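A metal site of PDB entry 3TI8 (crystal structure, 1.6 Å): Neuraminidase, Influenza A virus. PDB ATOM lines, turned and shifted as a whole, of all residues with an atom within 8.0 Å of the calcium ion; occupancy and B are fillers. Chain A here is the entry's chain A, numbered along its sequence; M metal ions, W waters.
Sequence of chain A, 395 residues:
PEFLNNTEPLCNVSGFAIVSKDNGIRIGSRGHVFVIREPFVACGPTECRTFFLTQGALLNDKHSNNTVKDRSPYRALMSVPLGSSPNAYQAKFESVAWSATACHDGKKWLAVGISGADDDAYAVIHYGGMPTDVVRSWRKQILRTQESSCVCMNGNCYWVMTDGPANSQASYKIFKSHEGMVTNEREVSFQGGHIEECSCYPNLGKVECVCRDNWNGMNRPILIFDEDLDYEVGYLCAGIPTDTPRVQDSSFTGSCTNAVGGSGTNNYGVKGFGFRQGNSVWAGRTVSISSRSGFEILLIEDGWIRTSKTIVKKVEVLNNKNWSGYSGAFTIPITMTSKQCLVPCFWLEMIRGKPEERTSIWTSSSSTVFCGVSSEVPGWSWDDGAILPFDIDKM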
ATOM      1  N   HIS A 194      11.625  30.336  14.893  1.00  0.00           N
ATOM      2  CA  HIS A 194      11.446  31.224  13.760  1.00  0.00           C
ATOM      3  C   HIS A 194      10.027  31.065  13.238  1.00  0.00           C
ATOM      4  O   HIS A 194       9.583  29.944  13.001  1.00  0.00           O
ATOM      5  CB  HIS A 194      12.465  30.892  12.663  1.00  0.00           C
ATOM      6  CG  HIS A 194      12.696  31.997  11.689  1.00  0.00           C
ATOM      7  ND1 HIS A 194      12.207  31.987  10.399  1.00  0.00           N
ATOM      8  CD2 HIS A 194      13.405  33.152  11.810  1.00  0.00           C
ATOM      9  CE1 HIS A 194      12.584  33.085   9.772  1.00  0.00           C
ATOM     10  NE2 HIS A 194      13.307  33.815  10.610  1.00  0.00           N
ATOM     11  N   CYS A 211       2.862  27.469  11.265  1.00  0.00           N
ATOM     12  CA  CYS A 211       3.693  28.423  10.538  1.00  0.00           C
ATOM     13  C   CYS A 211       4.900  27.792   9.857  1.00  0.00           C
ATOM     14  O   CYS A 211       5.018  26.564   9.777  1.00  0.00           O
ATOM     15  CB  CYS A 211       4.124  29.553  11.492  1.00  0.00           C
ATOM     16  SG  CYS A 211       2.758  30.220  12.520  1.00  0.00           S
ATOM     17  N   ARG A 212       5.783  28.648   9.349  1.00  0.00           N
ATOM     18  CA  ARG A 212       7.009  28.230   8.695  1.00  0.00           C
ATOM     19  C   ARG A 212       8.204  28.703   9.521  1.00  0.00           C
ATOM     20  O   ARG A 212       8.290  29.868   9.877  1.00  0.00           O
ATOM     21  CB  ARG A 212       7.080  28.833   7.291  1.00  0.00           C
ATOM     22  CG  ARG A 212       8.457  28.837   6.617  1.00  0.00           C
ATOM     23  CD  ARG A 212       8.380  29.617   5.296  1.00  0.00           C
ATOM     24  NE  ARG A 212       9.647  29.742   4.584  1.00  0.00           N
ATOM     25  CZ  ARG A 212       9.741  30.156   3.318  1.00  0.00           C
ATOM     26  NH1 ARG A 212       8.638  30.453   2.633  1.00  0.00           N
ATOM     27  NH2 ARG A 212      10.924  30.262   2.727  1.00  0.00           N
ATOM     28  N   ASP A 213       9.119  27.778   9.822  1.00  0.00           N
ATOM     29  CA  ASP A 213      10.383  28.129  10.457  1.00  0.00           C
ATOM     30  C   ASP A 213      11.421  28.138   9.358  1.00  0.00           C
ATOM     31  O   ASP A 213      11.665  27.112   8.739  1.00  0.00           O
ATOM     32  CB  ASP A 213      10.716  27.082  11.538  1.00  0.00           C
ATOM     33  CG  ASP A 213      12.046  27.346  12.233  1.00  0.00           C
ATOM     34  OD1 ASP A 213      13.053  27.602  11.545  1.00  0.00           O
ATOM     35  OD2 ASP A 213      12.090  27.270  13.484  1.00  0.00           O
ATOM     36  N   ASN A 214      12.023  29.290   9.072  1.00  0.00           N
ATOM     37  CA  ASN A 214      12.975  29.404   7.976  1.00  0.00           C
ATOM     38  C   ASN A 214      14.426  29.372   8.459  1.00  0.00           C
ATOM     39  O   ASN A 214      15.355  29.732   7.726  1.00  0.00           O
ATOM     40  CB  ASN A 214      12.727  30.707   7.192  1.00  0.00           C
ATOM     41  CG  ASN A 214      13.107  30.593   5.736  1.00  0.00           C
ATOM     42  OD1 ASN A 214      12.611  29.729   5.012  1.00  0.00           O
ATOM     43  ND2 ASN A 214      13.998  31.474   5.287  1.00  0.00           N
ATOM     44  N   TRP A 215      14.599  28.914   9.700  1.00  0.00           N
ATOM     45  CA  TRP A 215      15.885  28.955  10.388  1.00  0.00           C
ATOM     46  C   TRP A 215      16.323  27.524  10.690  1.00  0.00           C
ATOM     47  O   TRP A 215      16.790  26.816   9.803  1.00  0.00           O
ATOM     48  CB  TRP A 215      15.731  29.793  11.657  1.00  0.00           C
ATOM     49  CG  TRP A 215      16.986  30.030  12.454  1.00  0.00           C
ATOM     50  CD1 TRP A 215      18.276  29.796  12.065  1.00  0.00           C
ATOM     51  CD2 TRP A 215      17.065  30.572  13.782  1.00  0.00           C
ATOM     52  NE1 TRP A 215      19.142  30.146  13.078  1.00  0.00           N
ATOM     53  CE2 TRP A 215      18.425  30.630  14.139  1.00  0.00           C
ATOM     54  CE3 TRP A 215      16.106  31.013  14.698  1.00  0.00           C
ATOM     55  CZ2 TRP A 215      18.851  31.101  15.371  1.00  0.00           C
ATOM     56  CZ3 TRP A 215      16.526  31.479  15.925  1.00  0.00           C
ATOM     57  CH2 TRP A 215      17.884  31.531  16.253  1.00  0.00           C
ATOM     58  N   ASN A 216      16.120  27.069  11.927  1.00  0.00           N
ATOM     59  CA  ASN A 216      16.610  25.751  12.354  1.00  0.00           C
ATOM     60  C   ASN A 216      15.586  24.610  12.401  1.00  0.00           C
ATOM     61  O   ASN A 216      15.909  23.521  12.866  1.00  0.00           O
ATOM     62  CB  ASN A 216      17.299  25.870  13.718  1.00  0.00           C
ATOM     63  CG  ASN A 216      18.633  26.580  13.636  1.00  0.00           C
ATOM     64  OD1 ASN A 216      19.029  27.279  14.570  1.00  0.00           O
ATOM     65  ND2 ASN A 216      19.328  26.406  12.523  1.00  0.00           N
ATOM     66  N   GLY A 217      14.370  24.848  11.932  1.00  0.00           N
ATOM     67  CA  GLY A 217      13.322  23.848  12.094  1.00  0.00           C
ATOM     68  C   GLY A 217      12.718  23.304  10.817  1.00  0.00           C
ATOM     69  O   GLY A 217      12.267  24.065   9.956  1.00  0.00           O
ATOM     70  N   MET A 218      12.699  21.985  10.678  1.00  0.00           N
ATOM     71  CA  MET A 218      11.979  21.325   9.582  1.00  0.00           C
ATOM     72  C   MET A 218      10.603  20.886  10.102  1.00  0.00           C
ATOM     73  O   MET A 218       9.776  20.389   9.334  1.00  0.00           O
ATOM     74  CB  MET A 218      12.753  20.118   9.049  1.00  0.00           C
ATOM     75  CG  MET A 218      12.677  18.892   9.950  1.00  0.00           C
ATOM     76  SD  MET A 218      13.575  17.471   9.304  1.00  0.00           S
ATOM     77  CE  MET A 218      15.216  17.774   9.970  1.00  0.00           C
ATOM     78  N   ASN A 219      10.394  21.063  11.399  1.00  0.00           N
ATOM     79  CA  ASN A 219       9.053  20.987  11.968  1.00  0.00           C
ATOM     80  C   ASN A 219       8.428  22.381  12.005  1.00  0.00           C
ATOM     81  O   ASN A 219       9.136  23.389  11.974  1.00  0.00           O
ATOM     82  CB  ASN A 219       9.036  20.311  13.358  1.00  0.00           C
ATOM     83  CG  ASN A 219      10.067  20.889  14.339  1.00  0.00           C
ATOM     84  OD1 ASN A 219      10.973  21.630  13.952  1.00  0.00           O
ATOM     85  ND2 ASN A 219       9.936  20.537  15.609  1.00  0.00           N
ATOM     86  N   ARG A 220       7.102  22.428  12.045  1.00  0.00           N
ATOM     87  CA  ARG A 220       6.383  23.700  11.944  1.00  0.00           C
ATOM     88  C   ARG A 220       6.039  24.301  13.308  1.00  0.00           C
ATOM     89  O   ARG A 220       5.505  23.618  14.168  1.00  0.00           O
ATOM     90  CB  ARG A 220       5.109  23.529  11.127  1.00  0.00           C
ATOM     91  CG  ARG A 220       5.356  23.225   9.667  1.00  0.00           C
ATOM     92  CD  ARG A 220       4.094  23.448   8.841  1.00  0.00           C
ATOM     93  NE  ARG A 220       4.355  23.218   7.421  1.00  0.00           N
ATOM     94  CZ  ARG A 220       4.988  24.083   6.633  1.00  0.00           C
ATOM     95  NH1 ARG A 220       5.415  25.243   7.116  1.00  0.00           N
ATOM     96  NH2 ARG A 220       5.189  23.784   5.356  1.00  0.00           N
ATOM     97  N   PRO A 221       6.323  25.610  13.485  1.00  0.00           N
ATOM     98  CA  PRO A 221       5.885  26.280  14.710  1.00  0.00           C
ATOM     99  C   PRO A 221       4.370  26.251  14.851  1.00  0.00           C
ATOM    100  O   PRO A 221       3.639  26.310  13.847  1.00  0.00           O
ATOM    101  CB  PRO A 221       6.344  27.727  14.499  1.00  0.00           C
ATOM    102  CG  PRO A 221       7.469  27.632  13.524  1.00  0.00           C
ATOM    103  CD  PRO A 221       7.112  26.487  12.605  1.00  0.00           C
ATOM    104  N   TYR A 235       6.215  23.973  18.779  1.00  0.00           N
ATOM    105  CA  TYR A 235       6.229  23.293  17.490  1.00  0.00           C
ATOM    106  C   TYR A 235       5.179  22.194  17.416  1.00  0.00           C
ATOM    107  O   TYR A 235       4.760  21.655  18.442  1.00  0.00           O
ATOM    108  CB  TYR A 235       7.619  22.718  17.181  1.00  0.00           C
ATOM    109  CG  TYR A 235       8.613  23.779  16.821  1.00  0.00           C
ATOM    110  CD1 TYR A 235       9.281  24.502  17.806  1.00  0.00           C
ATOM    111  CD2 TYR A 235       8.873  24.090  15.488  1.00  0.00           C
ATOM    112  CE1 TYR A 235      10.184  25.499  17.471  1.00  0.00           C
ATOM    113  CE2 TYR A 235       9.775  25.087  15.153  1.00  0.00           C
ATOM    114  CZ  TYR A 235      10.415  25.781  16.145  1.00  0.00           C
ATOM    115  OH  TYR A 235      11.311  26.780  15.817  1.00  0.00           O
ATOM    116  N   ASP A 243       7.558  20.470   7.027  1.00  0.00           N
ATOM    117  CA  ASP A 243       8.130  21.579   6.262  1.00  0.00           C
ATOM    118  C   ASP A 243       8.841  20.993   5.047  1.00  0.00           C
ATOM    119  O   ASP A 243       8.952  19.777   4.928  1.00  0.00           O
ATOM    120  CB  ASP A 243       9.123  22.356   7.130  1.00  0.00           C
ATOM    121  CG  ASP A 243       9.410  23.755   6.600  1.00  0.00           C
ATOM    122  OD1 ASP A 243       8.778  24.198   5.621  1.00  0.00           O
ATOM    123  OD2 ASP A 243      10.283  24.424   7.201  1.00  0.00           O
ATOM    124  N   THR A 244       9.300  21.861   4.155  1.00  0.00           N
ATOM    125  CA  THR A 244      10.157  21.465   3.041  1.00  0.00           C
ATOM    126  C   THR A 244      11.214  22.550   2.896  1.00  0.00           C
ATOM    127  O   THR A 244      10.864  23.713   2.746  1.00  0.00           O
ATOM    128  CB  THR A 244       9.358  21.360   1.723  1.00  0.00           C
ATOM    129  OG1 THR A 244       8.214  20.517   1.924  1.00  0.00           O
ATOM    130  CG2 THR A 244      10.219  20.786   0.610  1.00  0.00           C
ATOM    131  N   PRO A 245      12.500  22.165   2.939  1.00  0.00           N
ATOM    132  CA  PRO A 245      13.033  20.799   3.005  1.00  0.00           C
ATOM    133  C   PRO A 245      12.928  20.141   4.374  1.00  0.00           C
ATOM    134  O   PRO A 245      12.768  20.809   5.390  1.00  0.00           O
ATOM    135  CB  PRO A 245      14.508  20.983   2.631  1.00  0.00           C
ATOM    136  CG  PRO A 245      14.840  22.353   3.098  1.00  0.00           C
ATOM    137  CD  PRO A 245      13.580  23.166   2.866  1.00  0.00           C
ATOM    138  N   ARG A 246      13.039  18.809   4.368  1.00  0.00           N
ATOM    139  CA  ARG A 246      13.000  18.001   5.580  1.00  0.00           C
ATOM    140  C   ARG A 246      13.711  16.690   5.280  1.00  0.00           C
ATOM    141  O   ARG A 246      14.181  16.476   4.166  1.00  0.00           O
ATOM    142  CB  ARG A 246      11.555  17.725   6.006  1.00  0.00           C
ATOM    143  CG  ARG A 246      10.748  16.948   4.966  1.00  0.00           C
ATOM    144  CD  ARG A 246       9.318  16.682   5.420  1.00  0.00           C
ATOM    145  NE  ARG A 246       8.648  15.788   4.473  1.00  0.00           N
ATOM    146  CZ  ARG A 246       8.001  16.188   3.388  1.00  0.00           C
ATOM    147  NH1 ARG A 246       7.882  17.483   3.122  1.00  0.00           N
ATOM    148  NH2 ARG A 246       7.444  15.293   2.583  1.00  0.00           N
ATOM    149  N   VAL A 260      13.600  21.304  15.250  1.00  0.00           N
ATOM    150  CA  VAL A 260      14.365  20.120  14.889  1.00  0.00           C
ATOM    151  C   VAL A 260      14.795  20.271  13.448  1.00  0.00           C
ATOM    152  O   VAL A 260      13.960  20.384  12.558  1.00  0.00           O
ATOM    153  CB  VAL A 260      13.518  18.836  15.046  1.00  0.00           C
ATOM    154  CG1 VAL A 260      14.306  17.613  14.602  1.00  0.00           C
ATOM    155  CG2 VAL A 260      13.038  18.707  16.489  1.00  0.00           C
ATOM    156  N   GLY A 261      16.107  20.274  13.211  1.00  0.00           N
ATOM    157  CA  GLY A 261      16.619  20.550  11.880  1.00  0.00           C
ATOM    158  C   GLY A 261      17.895  19.811  11.538  1.00  0.00           C
ATOM    159  O   GLY A 261      18.055  18.627  11.847  1.00  0.00           O
ATOM    160  N   THR A 265      18.606  20.724   5.985  1.00  0.00           N
ATOM    161  CA  THR A 265      17.260  21.280   5.942  1.00  0.00           C
ATOM    162  C   THR A 265      17.172  22.706   6.480  1.00  0.00           C
ATOM    163  O   THR A 265      16.135  23.364   6.348  1.00  0.00           O
ATOM    164  CB  THR A 265      16.252  20.403   6.718  1.00  0.00           C
ATOM    165  OG1 THR A 265      16.479  20.540   8.131  1.00  0.00           O
ATOM    166  CG2 THR A 265      16.378  18.945   6.312  1.00  0.00           C
ATOM    167  N   ASN A 266      18.244  23.193   7.107  1.00  0.00           N
ATOM    168  CA  ASN A 266      18.224  24.532   7.703  1.00  0.00           C
ATOM    169  C   ASN A 266      18.118  25.659   6.673  1.00  0.00           C
ATOM    170  O   ASN A 266      18.489  25.491   5.507  1.00  0.00           O
ATOM    171  CB  ASN A 266      19.457  24.770   8.579  1.00  0.00           C
ATOM    172  CG  ASN A 266      19.491  23.896   9.823  1.00  0.00           C
ATOM    173  OD1 ASN A 266      20.525  23.760  10.472  1.00  0.00           O
ATOM    174  ND2 ASN A 266      18.342  23.305  10.175  1.00  0.00           N
ATOM    175  N   ASN A 267      17.601  26.799   7.107  1.00  0.00           N
ATOM    176  CA  ASN A 267      17.644  28.036   6.328  1.00  0.00           C
ATOM    177  C   ASN A 267      16.688  28.108   5.141  1.00  0.00           C
ATOM    178  O   ASN A 267      16.849  28.970   4.267  1.00  0.00           O
ATOM    179  CB  ASN A 267      19.073  28.338   5.894  1.00  0.00           C
ATOM    180  CG  ASN A 267      19.999  28.510   7.066  1.00  0.00           C
ATOM    181  OD1 ASN A 267      19.642  29.153   8.049  1.00  0.00           O
ATOM    182  ND2 ASN A 267      21.190  27.929   6.988  1.00  0.00           N
ATOM    183  N   TYR A 268      15.695  27.227   5.101  1.00  0.00           N
ATOM    184  CA  TYR A 268      14.630  27.387   4.112  1.00  0.00           C
ATOM    185  C   TYR A 268      13.362  26.784   4.679  1.00  0.00           C
ATOM    186  O   TYR A 268      13.306  26.408   5.843  1.00  0.00           O
ATOM    187  CB  TYR A 268      14.999  26.757   2.766  1.00  0.00           C
ATOM    188  CG  TYR A 268      14.264  27.355   1.575  1.00  0.00           C
ATOM    189  CD1 TYR A 268      14.198  28.742   1.398  1.00  0.00           C
ATOM    190  CD2 TYR A 268      13.664  26.553   0.620  1.00  0.00           C
ATOM    191  CE1 TYR A 268      13.546  29.298   0.315  1.00  0.00           C
ATOM    192  CE2 TYR A 268      12.999  27.098  -0.474  1.00  0.00           C
ATOM    193  CZ  TYR A 268      12.948  28.472  -0.619  1.00  0.00           C
ATOM    194  OH  TYR A 268      12.299  29.041  -1.702  1.00  0.00           O
ATOM    195  N   GLY A 269      12.323  26.723   3.855  1.00  0.00           N
ATOM    196  CA  GLY A 269      11.030  26.250   4.308  1.00  0.00           C
ATOM    197  C   GLY A 269      10.007  26.577   3.251  1.00  0.00           C
ATOM    198  O   GLY A 269      10.342  27.084   2.176  1.00  0.00           O
ATOM    199  N   VAL A 270       8.752  26.277   3.543  1.00  0.00           N
ATOM    200  CA  VAL A 270       7.648  26.627   2.658  1.00  0.00           C
ATOM    201  C   VAL A 270       6.424  26.880   3.526  1.00  0.00           C
ATOM    202  O   VAL A 270       6.271  26.258   4.565  1.00  0.00           O
ATOM    203  CB  VAL A 270       7.361  25.505   1.632  1.00  0.00           C
ATOM    204  CG1 VAL A 270       6.815  24.260   2.311  1.00  0.00           C
ATOM    205  CG2 VAL A 270       6.406  26.006   0.545  1.00  0.00           C
HETATM  206 CA    CA M   1      12.462  25.118   7.754  1.00  0.00          CA
HETATM  207  O   HOH W   1      13.476  23.143   6.594  1.00  0.00           O
HETATM  208  O   HOH W   2      14.834  25.285   8.510  1.00  0.00           O
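The backbone carbonyl oxygen (O) of Gly 269 lies within hydrogen-bond range of the guanidinium group (NH2) of Arg 212, 3.3 Å away.
The side-chain carboxylate (OD1) of Asp 243 lies within salt-bridge range of the guanidinium group (NH2) of Arg 220 (3.6 Å).
N of Gly 269 sits at hydrogen-bond distance from OD1 of Asn 214.
The backbone carbonyl oxygen (O) of Tyr 268 sits close to the side-chain amide oxygen (OD1) of Asn 214, 3.5 Å away.
The backbone carbonyl oxygen of Met 218 sits close to the backbone NH of Asp 243, at 3.2 Å.
OD1 of Asp 213 is in hydrogen-bond range of N of Trp 215 (2.7 Å).
The backbone NH (N) of Gly 217 sits at hydrogen-bond distance from the side-chain carboxylate (OD1) of Asp 213 (3.1 Å).
The side-chain carboxylate (OD2) of Asp 213 sits at hydrogen-bond distance from the side-chain hydroxyl (OH) of Tyr 235, at 2.5 Å.
OD2 of Asp 243 binds the calcium ion, 2.4 Å away.
The backbone carbonyl oxygen (O) of Asp 213 binds the calcium ion (2.4 Å).
The calcium ion is bound by O of Gly 217, at 2.4 Å.
The calcium ion is bound by O of Tyr 268.
The calcium ion is bound by water W2, 2.5 Å away.
Water W1 binds the calcium ion, at 2.5 Å.
The calcium ion has six donor atoms within binding distance.
Gly 269 touches the calcium ion (CA to CA, 3.9 Å).
Five residues have an atom within 4 Å of the calcium ion: Asp 213, Gly 217, Asp 243, Tyr 268 and Gly 269.
Along chain A the residues within 4 Å of the calcium ion span positions 213 to 269.
The nearest printed residue that does not touch the calcium ion is Met 218 (4.2 Å).
Water W1 lies within hydrogen-bond range of O of Thr 265 and O of Pro 245.
Water W2 lies within hydrogen-bond range of the backbone carbonyl oxygen (O) of Trp 215 (2.8 Å), the backbone carbonyl oxygen (O) of Thr 265 (3.2 Å), the backbone NH (N) of Asn 267 (3.5 Å) and the backbone NH (N) of Gly 217 (3.5 Å).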
